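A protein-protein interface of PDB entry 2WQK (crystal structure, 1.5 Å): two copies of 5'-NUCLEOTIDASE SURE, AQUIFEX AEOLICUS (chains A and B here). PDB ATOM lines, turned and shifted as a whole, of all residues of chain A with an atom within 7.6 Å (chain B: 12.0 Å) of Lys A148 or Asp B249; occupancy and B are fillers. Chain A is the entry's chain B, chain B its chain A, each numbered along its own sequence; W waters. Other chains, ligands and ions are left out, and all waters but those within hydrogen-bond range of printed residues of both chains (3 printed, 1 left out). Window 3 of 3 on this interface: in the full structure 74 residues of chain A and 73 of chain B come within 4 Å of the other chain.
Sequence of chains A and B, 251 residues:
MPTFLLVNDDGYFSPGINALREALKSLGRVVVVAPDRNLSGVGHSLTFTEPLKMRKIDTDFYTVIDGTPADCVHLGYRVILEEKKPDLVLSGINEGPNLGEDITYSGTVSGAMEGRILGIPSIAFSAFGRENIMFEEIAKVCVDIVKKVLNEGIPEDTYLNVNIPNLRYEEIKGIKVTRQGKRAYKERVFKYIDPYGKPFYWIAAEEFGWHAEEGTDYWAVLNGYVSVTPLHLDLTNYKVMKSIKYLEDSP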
ATOM      1  N   LEU A  27      25.582  -0.506   9.989  1.00  0.00           N
ATOM      2  CA  LEU A  27      24.826  -0.618  11.242  1.00  0.00           C
ATOM      3  C   LEU A  27      25.710  -0.816  12.474  1.00  0.00           C
ATOM      4  O   LEU A  27      25.256  -0.682  13.600  1.00  0.00           O
ATOM      5  CB  LEU A  27      23.819  -1.800  11.195  1.00  0.00           C
ATOM      6  CG  LEU A  27      22.819  -1.716  10.070  1.00  0.00           C
ATOM      7  CD1 LEU A  27      21.834  -2.919  10.114  1.00  0.00           C
ATOM      8  CD2 LEU A  27      22.026  -0.411  10.078  1.00  0.00           C
ATOM      9  N   CYS A 142      18.555  -8.231   4.071  1.00  0.00           N
ATOM     10  CA  CYS A 142      19.081  -8.708   5.356  1.00  0.00           C
ATOM     11  C   CYS A 142      19.343  -7.546   6.304  1.00  0.00           C
ATOM     12  O   CYS A 142      19.045  -7.613   7.506  1.00  0.00           O
ATOM     13  CB  CYS A 142      20.334  -9.543   5.157  1.00  0.00           C
ATOM     14  SG  CYS A 142      20.063 -11.037   4.214  1.00  0.00           S
ATOM     15  N   VAL A 143      19.971  -6.491   5.763  1.00  0.00           N
ATOM     16  CA  VAL A 143      20.274  -5.321   6.569  1.00  0.00           C
ATOM     17  C   VAL A 143      18.988  -4.603   7.051  1.00  0.00           C
ATOM     18  O   VAL A 143      18.914  -4.161   8.187  1.00  0.00           O
ATOM     19  CB  VAL A 143      21.251  -4.357   5.846  1.00  0.00           C
ATOM     20  CG1 VAL A 143      21.295  -2.973   6.554  1.00  0.00           C
ATOM     21  CG2 VAL A 143      22.639  -5.057   5.693  1.00  0.00           C
ATOM     22  N   ASP A 144      17.960  -4.561   6.202  1.00  0.00           N
ATOM     23  CA  ASP A 144      16.668  -3.998   6.602  1.00  0.00           C
ATOM     24  C   ASP A 144      16.152  -4.745   7.850  1.00  0.00           C
ATOM     25  O   ASP A 144      15.684  -4.150   8.810  1.00  0.00           O
ATOM     26  CB  ASP A 144      15.624  -4.095   5.485  1.00  0.00           C
ATOM     27  CG  ASP A 144      15.868  -3.126   4.318  1.00  0.00           C
ATOM     28  OD1 ASP A 144      16.658  -2.170   4.470  1.00  0.00           O
ATOM     29  OD2 ASP A 144      15.258  -3.370   3.258  1.00  0.00           O
ATOM     30  N   ILE A 145      16.253  -6.068   7.812  1.00  0.00           N
ATOM     31  CA  ILE A 145      15.781  -6.889   8.937  1.00  0.00           C
ATOM     32  C   ILE A 145      16.596  -6.660  10.184  1.00  0.00           C
ATOM     33  O   ILE A 145      16.031  -6.474  11.260  1.00  0.00           O
ATOM     34  CB  ILE A 145      15.730  -8.380   8.502  1.00  0.00           C
ATOM     35  CG1 ILE A 145      14.587  -8.614   7.498  1.00  0.00           C
ATOM     36  CG2 ILE A 145      15.550  -9.299   9.736  1.00  0.00           C
ATOM     37  CD1 ILE A 145      14.669  -9.970   6.789  1.00  0.00           C
ATOM     38  N   VAL A 146      17.927  -6.636  10.040  1.00  0.00           N
ATOM     39  CA  VAL A 146      18.766  -6.443  11.213  1.00  0.00           C
ATOM     40  C   VAL A 146      18.455  -5.072  11.842  1.00  0.00           C
ATOM     41  O   VAL A 146      18.372  -4.944  13.070  1.00  0.00           O
ATOM     42  CB  VAL A 146      20.244  -6.554  10.846  1.00  0.00           C
ATOM     43  CG1 VAL A 146      21.124  -6.130  12.021  1.00  0.00           C
ATOM     44  CG2 VAL A 146      20.588  -8.027  10.380  1.00  0.00           C
ATOM     45  N   LYS A 147      18.282  -4.059  10.999  1.00  0.00           N
ATOM     46  CA  LYS A 147      17.974  -2.731  11.559  1.00  0.00           C
ATOM     47  C   LYS A 147      16.713  -2.759  12.430  1.00  0.00           C
ATOM     48  O   LYS A 147      16.701  -2.237  13.544  1.00  0.00           O
ATOM     49  CB  LYS A 147      17.830  -1.688  10.458  1.00  0.00           C
ATOM     50  CG  LYS A 147      17.773  -0.288  11.049  1.00  0.00           C
ATOM     51  CD  LYS A 147      17.708   0.757   9.949  1.00  0.00           C
ATOM     52  CE  LYS A 147      17.495   2.131  10.610  1.00  0.00           C
ATOM     53  NZ  LYS A 147      17.684   3.226   9.610  1.00  0.00           N
ATOM     54  N   LYS A 148      15.667  -3.430  11.937  1.00  0.00           N
ATOM     55  CA  LYS A 148      14.427  -3.514  12.675  1.00  0.00           C
ATOM     56  C   LYS A 148      14.579  -4.341  13.942  1.00  0.00           C
ATOM     57  O   LYS A 148      14.091  -3.972  15.012  1.00  0.00           O
ATOM     58  CB  LYS A 148      13.302  -4.084  11.798  1.00  0.00           C
ATOM     59  CG  LYS A 148      12.869  -3.163  10.613  1.00  0.00           C
ATOM     60  CD  LYS A 148      11.665  -3.768   9.885  1.00  0.00           C
ATOM     61  CE  LYS A 148      11.120  -2.871   8.758  1.00  0.00           C
ATOM     62  NZ  LYS A 148      10.463  -1.668   9.336  1.00  0.00           N
ATOM     63  N   VAL A 149      15.314  -5.438  13.858  1.00  0.00           N
ATOM     64  CA  VAL A 149      15.511  -6.274  15.038  1.00  0.00           C
ATOM     65  C   VAL A 149      16.301  -5.559  16.135  1.00  0.00           C
ATOM     66  O   VAL A 149      16.031  -5.712  17.326  1.00  0.00           O
ATOM     67  CB  VAL A 149      16.237  -7.590  14.649  1.00  0.00           C
ATOM     68  CG1 VAL A 149      16.754  -8.354  15.903  1.00  0.00           C
ATOM     69  CG2 VAL A 149      15.286  -8.453  13.801  1.00  0.00           C
ATOM     70  N   LEU A 150      17.294  -4.754  15.747  1.00  0.00           N
ATOM     71  CA  LEU A 150      18.035  -4.011  16.766  1.00  0.00           C
ATOM     72  C   LEU A 150      17.109  -3.052  17.506  1.00  0.00           C
ATOM     73  O   LEU A 150      17.335  -2.764  18.686  1.00  0.00           O
ATOM     74  CB  LEU A 150      19.130  -3.172  16.107  1.00  0.00           C
ATOM     75  CG  LEU A 150      20.350  -3.965  15.662  1.00  0.00           C
ATOM     76  CD1 LEU A 150      21.271  -3.113  14.684  1.00  0.00           C
ATOM     77  CD2 LEU A 150      21.187  -4.523  16.820  1.00  0.00           C
ATOM     78  N   ASN A 151      16.107  -2.547  16.799  1.00  0.00           N
ATOM     79  CA  ASN A 151      15.139  -1.623  17.399  1.00  0.00           C
ATOM     80  C   ASN A 151      14.079  -2.296  18.252  1.00  0.00           C
ATOM     81  O   ASN A 151      13.706  -1.781  19.295  1.00  0.00           O
ATOM     82  CB  ASN A 151      14.460  -0.793  16.313  1.00  0.00           C
ATOM     83  CG  ASN A 151      15.300   0.366  15.867  1.00  0.00           C
ATOM     84  OD1 ASN A 151      16.200   0.806  16.586  1.00  0.00           O
ATOM     85  ND2 ASN A 151      15.012   0.878  14.671  1.00  0.00           N
ATOM     86  N   GLU A 152      13.588  -3.459  17.831  1.00  0.00           N
ATOM     87  CA  GLU A 152      12.399  -4.014  18.460  1.00  0.00           C
ATOM     88  C   GLU A 152      12.625  -5.329  19.173  1.00  0.00           C
ATOM     89  O   GLU A 152      11.845  -5.682  20.041  1.00  0.00           O
ATOM     90  CB  GLU A 152      11.304  -4.210  17.426  1.00  0.00           C
ATOM     91  CG  GLU A 152      10.845  -2.925  16.734  1.00  0.00           C
ATOM     92  CD  GLU A 152      10.162  -1.941  17.664  1.00  0.00           C
ATOM     93  OE1 GLU A 152       9.694  -2.345  18.759  1.00  0.00           O
ATOM     94  OE2 GLU A 152      10.100  -0.743  17.299  1.00  0.00           O
ATOM     95  N   GLY A 153      13.646  -6.072  18.778  1.00  0.00           N
ATOM     96  CA  GLY A 153      14.041  -7.290  19.470  1.00  0.00           C
ATOM     97  C   GLY A 153      13.307  -8.549  19.023  1.00  0.00           C
ATOM     98  O   GLY A 153      12.350  -8.508  18.248  1.00  0.00           O
ATOM     99  N   ILE A 154      13.815  -9.674  19.525  1.00  0.00           N
ATOM    100  CA  ILE A 154      13.345 -11.053  19.154  1.00  0.00           C
ATOM    101  C   ILE A 154      12.803 -11.628  20.466  1.00  0.00           C
ATOM    102  O   ILE A 154      13.407 -11.423  21.522  1.00  0.00           O
ATOM    103  CB  ILE A 154      14.538 -11.934  18.618  1.00  0.00           C
ATOM    104  CG1 ILE A 154      15.149 -11.335  17.329  1.00  0.00           C
ATOM    105  CG2 ILE A 154      14.106 -13.441  18.320  1.00  0.00           C
ATOM    106  CD1 ILE A 154      16.388 -12.050  16.794  1.00  0.00           C
ATOM    107  N   ILE A 175       8.020  -8.812   3.007  1.00  0.00           N
ATOM    108  CA  ILE A 175       8.526  -9.744   4.033  1.00  0.00           C
ATOM    109  C   ILE A 175       7.318 -10.311   4.759  1.00  0.00           C
ATOM    110  O   ILE A 175       6.430  -9.568   5.202  1.00  0.00           O
ATOM    111  CB  ILE A 175       9.449  -8.988   5.029  1.00  0.00           C
ATOM    112  CG1 ILE A 175      10.676  -8.378   4.310  1.00  0.00           C
ATOM    113  CG2 ILE A 175       9.885  -9.907   6.217  1.00  0.00           C
ATOM    114  CD1 ILE A 175      11.485  -7.432   5.186  1.00  0.00           C
ATOM    115  N   MET B 241       4.692 -15.375  16.883  1.00  0.00           N
ATOM    116  CA  MET B 241       4.625 -14.756  15.554  1.00  0.00           C
ATOM    117  C   MET B 241       4.167 -13.308  15.607  1.00  0.00           C
ATOM    118  O   MET B 241       4.686 -12.435  14.881  1.00  0.00           O
ATOM    119  CB  MET B 241       3.721 -15.574  14.635  1.00  0.00           C
ATOM    120  CG  MET B 241       4.365 -16.843  14.239  1.00  0.00           C
ATOM    121  SD  MET B 241       3.254 -17.836  13.262  1.00  0.00           S
ATOM    122  CE  MET B 241       4.446 -18.853  12.423  1.00  0.00           C
ATOM    123  N   LYS B 242       3.187 -13.036  16.449  1.00  0.00           N
ATOM    124  CA  LYS B 242       2.628 -11.685  16.559  1.00  0.00           C
ATOM    125  C   LYS B 242       3.683 -10.651  16.960  1.00  0.00           C
ATOM    126  O   LYS B 242       3.601  -9.478  16.567  1.00  0.00           O
ATOM    127  CB  LYS B 242       1.450 -11.664  17.526  1.00  0.00           C
ATOM    128  CG  LYS B 242       1.776 -12.048  18.978  1.00  0.00           C
ATOM    129  CD  LYS B 242       0.511 -12.048  19.821  1.00  0.00           C
ATOM    130  CE  LYS B 242       0.752 -12.482  21.209  1.00  0.00           C
ATOM    131  NZ  LYS B 242       1.350 -13.846  21.353  1.00  0.00           N
ATOM    132  N   SER B 243       4.705 -11.103  17.695  1.00  0.00           N
ATOM    133  CA  SER B 243       5.732 -10.215  18.213  1.00  0.00           C
ATOM    134  C   SER B 243       6.863  -9.943  17.214  1.00  0.00           C
ATOM    135  O   SER B 243       7.738  -9.139  17.516  1.00  0.00           O
ATOM    136  CB  SER B 243       6.315 -10.776  19.503  1.00  0.00           C
ATOM    137  OG  SER B 243       5.318 -10.617  20.517  1.00  0.00           O
ATOM    138  N   ILE B 244       6.833 -10.571  16.038  1.00  0.00           N
ATOM    139  CA  ILE B 244       7.783 -10.246  14.993  1.00  0.00           C
ATOM    140  C   ILE B 244       7.076  -9.760  13.717  1.00  0.00           C
ATOM    141  O   ILE B 244       7.727  -9.571  12.682  1.00  0.00           O
ATOM    142  CB  ILE B 244       8.757 -11.395  14.709  1.00  0.00           C
ATOM    143  CG1 ILE B 244       8.032 -12.669  14.310  1.00  0.00           C
ATOM    144  CG2 ILE B 244       9.680 -11.632  15.938  1.00  0.00           C
ATOM    145  CD1 ILE B 244       8.967 -13.635  13.581  1.00  0.00           C
ATOM    146  N   LYS B 245       5.773  -9.477  13.800  1.00  0.00           N
ATOM    147  CA  LYS B 245       5.041  -8.978  12.636  1.00  0.00           C
ATOM    148  C   LYS B 245       5.517  -7.559  12.260  1.00  0.00           C
ATOM    149  O   LYS B 245       5.247  -7.105  11.128  1.00  0.00           O
ATOM    150  CB  LYS B 245       3.538  -8.990  12.915  1.00  0.00           C
ATOM    151  CG  LYS B 245       2.889 -10.384  12.777  1.00  0.00           C
ATOM    152  CD  LYS B 245       2.747 -10.801  11.299  1.00  0.00           C
ATOM    153  CE  LYS B 245       2.020 -12.129  11.085  1.00  0.00           C
ATOM    154  NZ  LYS B 245       2.529 -13.230  11.935  1.00  0.00           N
ATOM    155  N   TYR B 246       6.245  -6.885  13.154  1.00  0.00           N
ATOM    156  CA  TYR B 246       6.855  -5.601  12.799  1.00  0.00           C
ATOM    157  C   TYR B 246       7.805  -5.733  11.602  1.00  0.00           C
ATOM    158  O   TYR B 246       8.063  -4.765  10.892  1.00  0.00           O
ATOM    159  CB  TYR B 246       7.579  -4.986  13.998  1.00  0.00           C
ATOM    160  CG  TYR B 246       8.832  -5.716  14.445  1.00  0.00           C
ATOM    161  CD1 TYR B 246       8.802  -6.610  15.514  1.00  0.00           C
ATOM    162  CD2 TYR B 246      10.052  -5.496  13.825  1.00  0.00           C
ATOM    163  CE1 TYR B 246       9.941  -7.284  15.934  1.00  0.00           C
ATOM    164  CE2 TYR B 246      11.206  -6.175  14.239  1.00  0.00           C
ATOM    165  CZ  TYR B 246      11.150  -7.069  15.283  1.00  0.00           C
ATOM    166  OH  TYR B 246      12.322  -7.673  15.659  1.00  0.00           O
ATOM    167  N   LEU B 247       8.306  -6.951  11.348  1.00  0.00           N
ATOM    168  CA  LEU B 247       9.186  -7.167  10.230  1.00  0.00           C
ATOM    169  C   LEU B 247       8.479  -7.076   8.875  1.00  0.00           C
ATOM    170  O   LEU B 247       9.146  -6.924   7.855  1.00  0.00           O
ATOM    171  CB  LEU B 247       9.921  -8.519  10.371  1.00  0.00           C
ATOM    172  CG  LEU B 247      10.942  -8.593  11.492  1.00  0.00           C
ATOM    173  CD1 LEU B 247      11.456 -10.035  11.681  1.00  0.00           C
ATOM    174  CD2 LEU B 247      12.111  -7.656  11.225  1.00  0.00           C
ATOM    175  N   GLU B 248       7.159  -7.182   8.877  1.00  0.00           N
ATOM    176  CA  GLU B 248       6.360  -7.100   7.656  1.00  0.00           C
ATOM    177  C   GLU B 248       6.070  -5.643   7.254  1.00  0.00           C
ATOM    178  O   GLU B 248       5.640  -5.383   6.106  1.00  0.00           O
ATOM    179  CB  GLU B 248       5.052  -7.836   7.828  1.00  0.00           C
ATOM    180  CG  GLU B 248       5.187  -9.264   8.241  1.00  0.00           C
ATOM    181  CD  GLU B 248       3.890 -10.024   8.122  1.00  0.00           C
ATOM    182  OE1 GLU B 248       2.805  -9.368   8.107  1.00  0.00           O
ATOM    183  OE2 GLU B 248       3.922 -11.278   8.043  1.00  0.00           O
ATOM    184  N   ASP B 249       6.317  -4.712   8.165  1.00  0.00           N
ATOM    185  CA  ASP B 249       5.941  -3.293   7.929  1.00  0.00           C
ATOM    186  C   ASP B 249       6.848  -2.695   6.863  1.00  0.00           C
ATOM    187  O   ASP B 249       8.070  -2.681   6.994  1.00  0.00           O
ATOM    188  CB  ASP B 249       6.041  -2.479   9.217  1.00  0.00           C
ATOM    189  CG  ASP B 249       5.037  -2.917  10.287  1.00  0.00           C
ATOM    190  OD1 ASP B 249       4.089  -3.676   9.973  1.00  0.00           O
ATOM    191  OD2 ASP B 249       5.198  -2.489  11.461  1.00  0.00           O
HETATM  192  O   HOH W   1       8.877  -2.116  11.343  1.00  0.00           O
HETATM  193  O   HOH W   2       6.655  -6.300   3.683  1.00  0.00           O
HETATM  194  O   HOH W   3       9.405  -0.220   6.664  1.00  0.00           O
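The side-chain hydroxyl (OH) of Tyr B246 sits at hydrogen-bond distance from the backbone carbonyl oxygen (O) of Gly A153 (2.7 Å).
The backbone carbonyl oxygen of Asp B249 lies within hydrogen-bond range of the side-chain amino group of Lys A148, 3.5 Å away.
Among the printed residues, merely in contact across the chains: Lys A148 with Tyr B246 (3.7 Å), Lys A148 with Leu B247 (3.8 Å), Val A149 with Tyr B246 (3.5 Å), Glu A152 with Tyr B246 (3.6 Å), Ile A175 with Leu B247 (3.5 Å) and Ile A175 with Glu B248 (3.3 Å).
Asp A144 touches none of the printed residues of chain B.
No residue of chain B comes within 4 Å of Lys A147.
Of chain B, only Tyr B246, Leu B247 and Asp B249 come within 4 Å of Lys A148.
Printed residues of chain B within 4 Å of Val A149: Tyr B246 (3.5 Å).
No residue of chain B comes within 4 Å of Leu A150.
Of the printed residues of chain B, Glu A152 touches Tyr B246.
Gly A153 touches just one residue of chain B: Tyr B246 (2.7 Å).
Of chain B, only Leu B247 (3.5 Å) and Glu B248 (3.3 Å) come within 4 Å of Ile A175.
Printed residues of chain A within 4 Å of Leu B247: Lys A148 and Ile A175.
Printed residues of chain A within 4 Å of Glu B248: Ile A175.
Asp B249 touches one residue of chain A.
The nearest residue of chain B that does not touch Lys A148 is Glu B248 (5.7 Å).
The nearest printed residue of chain A that does not touch Leu B247 is Ile A145 (4.1 Å).
Printed residues of chain B that touch a printed residue of chain A: Tyr B246, Leu B247, Glu B248 and Asp B249.
Printed residues of chain A that touch a printed residue of chain B: Lys A148, Val A149, Glu A152, Gly A153 and Ile A175.
Hydrophobic or aromatic side chains of chain A that line the printed part of chain B: Val A149 and Ile A175.
Among the printed residues, 8 pairs touch across the chains.
Among the printed residues, no Asp or Glu carboxylate lies within 4 Å of a Lys or Arg side-chain nitrogen of the other chain.
No position is printed for both chains.
Of the 8 pairs that touch across the chains among the printed residues, none has its exchanged pair printed and touching as well.
Water W1 lies within hydrogen-bond range of the side-chain amino group (NZ) of Lys A148 (2.6 Å) and the backbone carbonyl oxygen (O) of Tyr B246 (2.8 Å).
Water W2 bridges O of Glu B248 (2.8 Å) and N of Ile A175 (2.9 Å).
Water W3 bridges O of Asp B249 (2.8 Å) and NZ of Lys A148 (3.2 Å).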
